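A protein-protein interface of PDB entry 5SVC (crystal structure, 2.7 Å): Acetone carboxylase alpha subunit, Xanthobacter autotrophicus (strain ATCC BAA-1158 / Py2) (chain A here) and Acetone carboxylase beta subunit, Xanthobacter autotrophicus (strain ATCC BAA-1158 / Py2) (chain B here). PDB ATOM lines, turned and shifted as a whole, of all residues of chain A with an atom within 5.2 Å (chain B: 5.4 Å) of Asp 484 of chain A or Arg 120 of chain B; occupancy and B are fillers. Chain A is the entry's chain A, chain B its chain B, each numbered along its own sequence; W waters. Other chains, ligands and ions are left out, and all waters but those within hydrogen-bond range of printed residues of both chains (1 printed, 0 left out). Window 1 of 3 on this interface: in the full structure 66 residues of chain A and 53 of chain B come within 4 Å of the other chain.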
ATOM      1  N   GLN A  86     -23.860  36.763  21.415  1.00  0.00           N
ATOM      2  CA  GLN A  86     -23.687  35.353  21.744  1.00  0.00           C
ATOM      3  C   GLN A  86     -22.383  35.069  22.486  1.00  0.00           C
ATOM      4  O   GLN A  86     -22.405  34.337  23.489  1.00  0.00           O
ATOM      5  CB  GLN A  86     -23.779  34.496  20.474  1.00  0.00           C
ATOM      6  CG  GLN A  86     -24.312  33.101  20.730  1.00  0.00           C
ATOM      7  CD  GLN A  86     -24.298  32.222  19.493  1.00  0.00           C
ATOM      8  OE1 GLN A  86     -23.488  32.417  18.590  1.00  0.00           O
ATOM      9  NE2 GLN A  86     -25.161  31.213  19.473  1.00  0.00           N
ATOM     10  N   GLU A  87     -21.255  35.654  22.040  1.00  0.00           N
ATOM     11  CA  GLU A  87     -19.949  35.383  22.650  1.00  0.00           C
ATOM     12  C   GLU A  87     -19.740  36.090  23.987  1.00  0.00           C
ATOM     13  O   GLU A  87     -19.004  35.582  24.832  1.00  0.00           O
ATOM     14  CB  GLU A  87     -18.806  35.785  21.704  1.00  0.00           C
ATOM     15  CG  GLU A  87     -19.052  35.577  20.210  1.00  0.00           C
ATOM     16  CD  GLU A  87     -19.331  34.152  19.884  1.00  0.00           C
ATOM     17  OE1 GLU A  87     -18.726  33.293  20.551  1.00  0.00           O
ATOM     18  OE2 GLU A  87     -20.169  33.891  18.993  1.00  0.00           O
ATOM     19  N   PHE A 456     -15.072  35.741  15.920  1.00  0.00           N
ATOM     20  CA  PHE A 456     -14.632  35.354  17.253  1.00  0.00           C
ATOM     21  C   PHE A 456     -14.675  33.840  17.465  1.00  0.00           C
ATOM     22  O   PHE A 456     -14.944  33.369  18.579  1.00  0.00           O
ATOM     23  CB  PHE A 456     -15.439  36.114  18.309  1.00  0.00           C
ATOM     24  CG  PHE A 456     -14.743  37.376  18.768  1.00  0.00           C
ATOM     25  CD1 PHE A 456     -14.591  38.442  17.901  1.00  0.00           C
ATOM     26  CD2 PHE A 456     -14.185  37.468  20.021  1.00  0.00           C
ATOM     27  CE1 PHE A 456     -13.913  39.571  18.282  1.00  0.00           C
ATOM     28  CE2 PHE A 456     -13.495  38.596  20.396  1.00  0.00           C
ATOM     29  CZ  PHE A 456     -13.374  39.649  19.529  1.00  0.00           C
ATOM     30  N   GLU A 457     -14.397  33.069  16.404  1.00  0.00           N
ATOM     31  CA  GLU A 457     -14.100  31.644  16.541  1.00  0.00           C
ATOM     32  C   GLU A 457     -12.824  31.407  17.354  1.00  0.00           C
ATOM     33  O   GLU A 457     -12.753  30.437  18.119  1.00  0.00           O
ATOM     34  CB  GLU A 457     -14.000  30.991  15.149  1.00  0.00           C
ATOM     35  CG  GLU A 457     -15.389  30.621  14.541  1.00  0.00           C
ATOM     36  CD  GLU A 457     -15.327  29.701  13.300  1.00  0.00           C
ATOM     37  OE1 GLU A 457     -14.497  29.935  12.398  1.00  0.00           O
ATOM     38  OE2 GLU A 457     -16.101  28.713  13.242  1.00  0.00           O
ATOM     39  N   ALA A 459     -12.171  32.687  19.991  1.00  0.00           N
ATOM     40  CA  ALA A 459     -12.459  32.669  21.418  1.00  0.00           C
ATOM     41  C   ALA A 459     -12.341  31.262  22.001  1.00  0.00           C
ATOM     42  O   ALA A 459     -12.359  31.112  23.229  1.00  0.00           O
ATOM     43  CB  ALA A 459     -13.856  33.237  21.681  1.00  0.00           C
ATOM     44  N   ALA A 460     -12.202  30.249  21.135  1.00  0.00           N
ATOM     45  CA  ALA A 460     -12.276  28.827  21.473  1.00  0.00           C
ATOM     46  C   ALA A 460     -11.054  28.101  20.899  1.00  0.00           C
ATOM     47  O   ALA A 460     -11.142  27.165  20.104  1.00  0.00           O
ATOM     48  CB  ALA A 460     -13.565  28.194  20.951  1.00  0.00           C
ATOM     49  N   ALA A 475     -11.756  25.704  23.414  1.00  0.00           N
ATOM     50  CA  ALA A 475     -12.340  25.925  24.736  1.00  0.00           C
ATOM     51  C   ALA A 475     -12.224  27.349  25.275  1.00  0.00           C
ATOM     52  O   ALA A 475     -13.146  27.820  25.952  1.00  0.00           O
ATOM     53  CB  ALA A 475     -11.687  24.928  25.729  1.00  0.00           C
ATOM     54  N   GLU A 482     -14.384  31.899  29.406  1.00  0.00           N
ATOM     55  CA  GLU A 482     -15.675  31.301  29.068  1.00  0.00           C
ATOM     56  C   GLU A 482     -15.790  31.217  27.553  1.00  0.00           C
ATOM     57  O   GLU A 482     -16.404  32.054  26.892  1.00  0.00           O
ATOM     58  CB  GLU A 482     -16.802  32.117  29.662  1.00  0.00           C
ATOM     59  CG  GLU A 482     -16.706  32.251  31.158  1.00  0.00           C
ATOM     60  CD  GLU A 482     -17.652  33.305  31.653  1.00  0.00           C
ATOM     61  OE1 GLU A 482     -18.861  33.003  31.799  1.00  0.00           O
ATOM     62  OE2 GLU A 482     -17.169  34.449  31.835  1.00  0.00           O
ATOM     63  N   GLY A 483     -15.167  30.183  27.002  1.00  0.00           N
ATOM     64  CA  GLY A 483     -15.099  30.061  25.561  1.00  0.00           C
ATOM     65  C   GLY A 483     -16.461  29.869  24.919  1.00  0.00           C
ATOM     66  O   GLY A 483     -17.378  29.270  25.486  1.00  0.00           O
ATOM     67  N   ASP A 484     -16.564  30.350  23.688  1.00  0.00           N
ATOM     68  CA  ASP A 484     -17.778  30.217  22.904  1.00  0.00           C
ATOM     69  C   ASP A 484     -17.391  30.292  21.439  1.00  0.00           C
ATOM     70  O   ASP A 484     -16.785  31.287  21.021  1.00  0.00           O
ATOM     71  CB  ASP A 484     -18.743  31.329  23.268  1.00  0.00           C
ATOM     72  CG  ASP A 484     -20.112  31.164  22.619  1.00  0.00           C
ATOM     73  OD1 ASP A 484     -20.202  30.668  21.480  1.00  0.00           O
ATOM     74  OD2 ASP A 484     -21.118  31.505  23.280  1.00  0.00           O
ATOM     75  N   MET A 485     -17.723  29.270  20.650  1.00  0.00           N
ATOM     76  CA  MET A 485     -17.428  29.476  19.236  1.00  0.00           C
ATOM     77  C   MET A 485     -18.598  30.103  18.478  1.00  0.00           C
ATOM     78  O   MET A 485     -18.399  30.677  17.399  1.00  0.00           O
ATOM     79  CB  MET A 485     -16.930  28.180  18.562  1.00  0.00           C
ATOM     80  CG  MET A 485     -17.829  26.966  18.527  1.00  0.00           C
ATOM     81  SD  MET A 485     -17.060  25.730  17.450  1.00  0.00           S
ATOM     82  CE  MET A 485     -16.162  24.694  18.619  1.00  0.00           C
ATOM     83  N   GLY A 486     -19.786  30.114  19.055  1.00  0.00           N
ATOM     84  CA  GLY A 486     -20.901  30.738  18.375  1.00  0.00           C
ATOM     85  C   GLY A 486     -21.421  29.811  17.307  1.00  0.00           C
ATOM     86  O   GLY A 486     -20.661  29.031  16.718  1.00  0.00           O
ATOM     87  N   ASP A 487     -22.708  29.905  17.021  1.00  0.00           N
ATOM     88  CA  ASP A 487     -23.320  28.981  16.083  1.00  0.00           C
ATOM     89  C   ASP A 487     -22.999  29.350  14.643  1.00  0.00           C
ATOM     90  O   ASP A 487     -22.919  30.529  14.282  1.00  0.00           O
ATOM     91  CB  ASP A 487     -24.826  28.943  16.287  1.00  0.00           C
ATOM     92  CG  ASP A 487     -25.230  28.021  17.419  1.00  0.00           C
ATOM     93  OD1 ASP A 487     -25.105  26.777  17.258  1.00  0.00           O
ATOM     94  OD2 ASP A 487     -25.676  28.545  18.468  1.00  0.00           O
ATOM     95  N   ARG A 502     -16.445  22.408   9.819  1.00  0.00           N
ATOM     96  CA  ARG A 502     -16.035  22.768  11.165  1.00  0.00           C
ATOM     97  C   ARG A 502     -15.497  21.478  11.739  1.00  0.00           C
ATOM     98  O   ARG A 502     -16.151  20.433  11.631  1.00  0.00           O
ATOM     99  CB  ARG A 502     -17.177  23.329  12.035  1.00  0.00           C
ATOM    100  CG  ARG A 502     -17.012  24.810  12.444  1.00  0.00           C
ATOM    101  CD  ARG A 502     -18.128  25.311  13.378  1.00  0.00           C
ATOM    102  NE  ARG A 502     -17.919  26.704  13.791  1.00  0.00           N
ATOM    103  CZ  ARG A 502     -18.591  27.323  14.769  1.00  0.00           C
ATOM    104  NH1 ARG A 502     -19.535  26.679  15.443  1.00  0.00           N
ATOM    105  NH2 ARG A 502     -18.320  28.592  15.085  1.00  0.00           N
ATOM    106  N   PHE B 115     -19.640  19.084  14.986  1.00  0.00           N
ATOM    107  CA  PHE B 115     -20.059  20.211  15.805  1.00  0.00           C
ATOM    108  C   PHE B 115     -20.762  19.744  17.074  1.00  0.00           C
ATOM    109  O   PHE B 115     -20.467  20.263  18.155  1.00  0.00           O
ATOM    110  CB  PHE B 115     -20.829  21.254  14.960  1.00  0.00           C
ATOM    111  CG  PHE B 115     -22.283  20.983  14.697  1.00  0.00           C
ATOM    112  CD1 PHE B 115     -23.249  21.320  15.636  1.00  0.00           C
ATOM    113  CD2 PHE B 115     -22.711  20.578  13.431  1.00  0.00           C
ATOM    114  CE1 PHE B 115     -24.603  21.151  15.358  1.00  0.00           C
ATOM    115  CE2 PHE B 115     -24.065  20.422  13.144  1.00  0.00           C
ATOM    116  CZ  PHE B 115     -25.006  20.688  14.103  1.00  0.00           C
ATOM    117  N   HIS B 116     -21.575  18.698  17.005  1.00  0.00           N
ATOM    118  CA  HIS B 116     -22.140  18.135  18.230  1.00  0.00           C
ATOM    119  C   HIS B 116     -21.081  17.932  19.323  1.00  0.00           C
ATOM    120  O   HIS B 116     -21.155  18.537  20.398  1.00  0.00           O
ATOM    121  CB  HIS B 116     -22.860  16.821  17.928  1.00  0.00           C
ATOM    122  CG  HIS B 116     -23.627  16.295  19.093  1.00  0.00           C
ATOM    123  ND1 HIS B 116     -24.522  17.080  19.802  1.00  0.00           N
ATOM    124  CD2 HIS B 116     -23.652  15.068  19.671  1.00  0.00           C
ATOM    125  CE1 HIS B 116     -25.048  16.360  20.779  1.00  0.00           C
ATOM    126  NE2 HIS B 116     -24.544  15.136  20.717  1.00  0.00           N
ATOM    127  N   MET B 118     -18.147  19.068  19.633  1.00  0.00           N
ATOM    128  CA  MET B 118     -17.355  20.206  20.084  1.00  0.00           C
ATOM    129  C   MET B 118     -18.111  21.057  21.109  1.00  0.00           C
ATOM    130  O   MET B 118     -17.511  21.954  21.721  1.00  0.00           O
ATOM    131  CB  MET B 118     -16.896  21.067  18.900  1.00  0.00           C
ATOM    132  CG  MET B 118     -15.757  20.464  18.072  1.00  0.00           C
ATOM    133  SD  MET B 118     -15.163  21.572  16.797  1.00  0.00           S
ATOM    134  CE  MET B 118     -16.723  22.047  16.070  1.00  0.00           C
ATOM    135  N   GLY B 119     -19.416  20.823  21.282  1.00  0.00           N
ATOM    136  CA  GLY B 119     -20.188  21.487  22.310  1.00  0.00           C
ATOM    137  C   GLY B 119     -20.194  22.990  22.236  1.00  0.00           C
ATOM    138  O   GLY B 119     -20.445  23.651  23.247  1.00  0.00           O
ATOM    139  N   ARG B 120     -19.889  23.552  21.066  1.00  0.00           N
ATOM    140  CA  ARG B 120     -19.778  25.000  20.828  1.00  0.00           C
ATOM    141  C   ARG B 120     -18.838  25.679  21.839  1.00  0.00           C
ATOM    142  O   ARG B 120     -18.874  26.897  21.999  1.00  0.00           O
ATOM    143  CB  ARG B 120     -21.163  25.692  20.778  1.00  0.00           C
ATOM    144  CG  ARG B 120     -21.114  27.123  20.145  1.00  0.00           C
ATOM    145  CD  ARG B 120     -22.427  27.756  19.787  1.00  0.00           C
ATOM    146  NE  ARG B 120     -23.410  27.751  20.869  1.00  0.00           N
ATOM    147  CZ  ARG B 120     -23.390  28.556  21.922  1.00  0.00           C
ATOM    148  NH1 ARG B 120     -22.413  29.424  22.077  1.00  0.00           N
ATOM    149  NH2 ARG B 120     -24.329  28.468  22.845  1.00  0.00           N
ATOM    150  N   ALA B 121     -17.953  24.902  22.479  1.00  0.00           N
ATOM    151  CA  ALA B 121     -16.993  25.372  23.480  1.00  0.00           C
ATOM    152  C   ALA B 121     -17.668  25.689  24.809  1.00  0.00           C
ATOM    153  O   ALA B 121     -17.291  25.137  25.850  1.00  0.00           O
ATOM    154  CB  ALA B 121     -16.235  26.608  22.974  1.00  0.00           C
ATOM    155  N   VAL B 122     -18.658  26.585  24.764  1.00  0.00           N
ATOM    156  CA  VAL B 122     -19.625  26.847  25.819  1.00  0.00           C
ATOM    157  C   VAL B 122     -19.794  25.676  26.775  1.00  0.00           C
ATOM    158  O   VAL B 122     -19.519  25.809  27.968  1.00  0.00           O
ATOM    159  CB  VAL B 122     -20.971  27.224  25.180  1.00  0.00           C
ATOM    160  CG1 VAL B 122     -22.093  27.057  26.155  1.00  0.00           C
ATOM    161  CG2 VAL B 122     -20.920  28.644  24.692  1.00  0.00           C
ATOM    162  N   GLN B 123     -20.228  24.515  26.273  1.00  0.00           N
ATOM    163  CA  GLN B 123     -20.610  23.427  27.213  1.00  0.00           C
ATOM    164  C   GLN B 123     -19.452  22.879  28.006  1.00  0.00           C
ATOM    165  O   GLN B 123     -19.649  21.841  28.676  1.00  0.00           O
ATOM    166  CB  GLN B 123     -21.291  22.252  26.494  1.00  0.00           C
ATOM    167  CG  GLN B 123     -22.679  22.505  25.926  1.00  0.00           C
ATOM    168  CD  GLN B 123     -23.076  21.400  24.992  1.00  0.00           C
ATOM    169  OE1 GLN B 123     -24.246  21.261  24.599  1.00  0.00           O
ATOM    170  NE2 GLN B 123     -22.087  20.578  24.632  1.00  0.00           N
ATOM    171  N   HIS B 125     -18.390  24.839  30.332  1.00  0.00           N
ATOM    172  CA  HIS B 125     -18.519  25.665  31.529  1.00  0.00           C
ATOM    173  C   HIS B 125     -19.961  26.084  31.800  1.00  0.00           C
ATOM    174  O   HIS B 125     -20.217  26.926  32.674  1.00  0.00           O
ATOM    175  CB  HIS B 125     -17.613  26.900  31.433  1.00  0.00           C
ATOM    176  CG  HIS B 125     -17.832  27.752  30.214  1.00  0.00           C
ATOM    177  ND1 HIS B 125     -18.792  28.745  30.158  1.00  0.00           N
ATOM    178  CD2 HIS B 125     -17.167  27.805  29.030  1.00  0.00           C
ATOM    179  CE1 HIS B 125     -18.724  29.352  28.982  1.00  0.00           C
ATOM    180  NE2 HIS B 125     -17.749  28.801  28.280  1.00  0.00           N
ATOM    181  N   THR B 235     -26.593  24.216  17.339  1.00  0.00           N
ATOM    182  CA  THR B 235     -26.241  23.405  18.500  1.00  0.00           C
ATOM    183  C   THR B 235     -27.437  23.231  19.420  1.00  0.00           C
ATOM    184  O   THR B 235     -27.610  22.157  20.020  1.00  0.00           O
ATOM    185  CB  THR B 235     -25.062  24.017  19.272  1.00  0.00           C
ATOM    186  OG1 THR B 235     -25.275  25.418  19.463  1.00  0.00           O
ATOM    187  CG2 THR B 235     -23.716  23.766  18.568  1.00  0.00           C
ATOM    188  N   HIS B 236     -28.253  24.294  19.558  1.00  0.00           N
ATOM    189  CA  HIS B 236     -29.474  24.238  20.364  1.00  0.00           C
ATOM    190  C   HIS B 236     -30.500  23.302  19.735  1.00  0.00           C
ATOM    191  O   HIS B 236     -31.081  22.443  20.411  1.00  0.00           O
ATOM    192  CB  HIS B 236     -30.068  25.643  20.517  1.00  0.00           C
ATOM    193  CG  HIS B 236     -29.242  26.579  21.341  1.00  0.00           C
ATOM    194  ND1 HIS B 236     -29.539  26.870  22.655  1.00  0.00           N
ATOM    195  CD2 HIS B 236     -28.130  27.291  21.042  1.00  0.00           C
ATOM    196  CE1 HIS B 236     -28.649  27.725  23.127  1.00  0.00           C
ATOM    197  NE2 HIS B 236     -27.782  27.995  22.170  1.00  0.00           N
ATOM    198  N   VAL B 347     -27.060  23.018  25.574  1.00  0.00           N
ATOM    199  CA  VAL B 347     -27.818  24.156  25.068  1.00  0.00           C
ATOM    200  C   VAL B 347     -29.091  23.617  24.436  1.00  0.00           C
ATOM    201  O   VAL B 347     -29.090  22.537  23.840  1.00  0.00           O
ATOM    202  CB  VAL B 347     -26.989  24.980  24.070  1.00  0.00           C
ATOM    203  CG1 VAL B 347     -25.912  25.658  24.797  1.00  0.00           C
ATOM    204  CG2 VAL B 347     -26.397  24.094  22.987  1.00  0.00           C
HETATM  205  O   HOH W   1     -19.959  30.021  32.157  1.00  0.00           O
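Ala 460 of chain A touches Ala 121 of chain B (CB to CB, 3.7 Å). Glu 482 of chain A touches His 125 of chain B. Gly 483 of chain A touches Ala 121 of chain B. Ala 121 of chain B touches Asp 484 of chain A (CB to N, 3.8 Å). OD2 of Asp 484 of chain A touches CG2 of Val 122 of chain B, at 3.2 Å. Met 485 of chain A touches Met 118 of chain B (CE to CB, 3.7 Å). Met 485 of chain A touches Ala 121 of chain B (N to CB, 3.8 Å). C of Gly 486 of chain A touches CD of Arg 120 of chain B (3.4 Å). CD2 of His 236 of chain B touches OD2 of Asp 487 of chain A, 3.8 Å away.
Water W1 bridges a ring nitrogen (ND1) of His 125 of chain B (2.6 Å) and the side-chain carboxylate of Glu 482 of chain A (3.2 Å).
Gln 86 of chain A touches none of the printed residues of chain B. Printed residues of chain B within 4 Å of Ala 460 of chain A: Ala 121. Ala 475 of chain A touches none of the printed residues of chain B. Printed residues of chain A within 4 Å of Val 122 of chain B: Gly 483 (3.1 Å) and Asp 484 (3.2 Å). The nearest residue of chain A that does not touch Arg 120 of chain B is Gln 86 of chain A (4.02 Å). The nearest printed residue of chain B that does not touch Gly 486 of chain A is Val 122 of chain B (5.9 Å).
The side-chain amide nitrogen of Gln 86 of chain A sits at hydrogen-bond distance from the side-chain carboxylate of Asp 487 of chain A (2.9 Å). OD1 of Asp 484 of chain A is in hydrogen-bond range of N of Gly 486 of chain A, at 2.5 Å. The guanidinium group (NH2) of Arg 502 of chain A is in hydrogen-bond range of the backbone carbonyl oxygen (O) of Met 485 of chain A (3.1 Å). O of Gly 486 of chain A lies within hydrogen-bond range of NH2 of Arg 502 of chain A, at 2.9 Å. The guanidinium group (NE) of Arg 120 of chain B sits at hydrogen-bond distance from the side-chain hydroxyl (OG1) of Thr 235 of chain B. The backbone carbonyl oxygen (O) of Val 122 of chain B sits close to a ring nitrogen (NE2) of His 125 of chain B (3.5 Å).
Printed residues of chain B that touch a printed residue of chain A: Met 118, Arg 120, Ala 121, Val 122, His 125, Thr 235 and His 236. Hydrophobic or aromatic side chains of chain B within 4 Å of the printed part of chain A: Met 118, Ala 121, Val 122, His 125 and His 236. Printed residues of chain A that touch a printed residue of chain B: Ala 460, Glu 482, Gly 483, Asp 484, Met 485, Gly 486 and Asp 487. Hydrophobic or aromatic side chains of chain A within 4 Å of the printed part of chain B: Ala 460 and Met 485. Among the printed residues, Asp or Glu carboxylates within 4 Å of a Lys or Arg side-chain nitrogen of the other chain: Asp 484 of chain A with Arg 120 of chain B (2.6 Å) and Asp 487 of chain A with Arg 120 of chain B (3.4 Å).
The backbone NH (N) of Val 122 of chain B is in hydrogen-bond range of the backbone carbonyl oxygen (O) of Gly 483 of chain A (3.1 Å). A ring nitrogen (NE2) of His 125 of chain B is in hydrogen-bond range of the backbone carbonyl oxygen of Gly 483 of chain A. The side-chain carboxylate (OD1) of Asp 484 of chain A is in salt-bridge range of the guanidinium group (NH1) of Arg 120 of chain B, at 2.6 Å. N of Met 485 of chain A is in hydrogen-bond range of O of Arg 120 of chain B, 3.0 Å away. NE of Arg 120 of chain B is in salt-bridge range of OD2 of Asp 487 of chain A (3.4 Å). The side-chain hydroxyl (OG1) of Thr 235 of chain B is in hydrogen-bond range of the side-chain carboxylate (OD1) of Asp 487 of chain A (2.6 Å).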
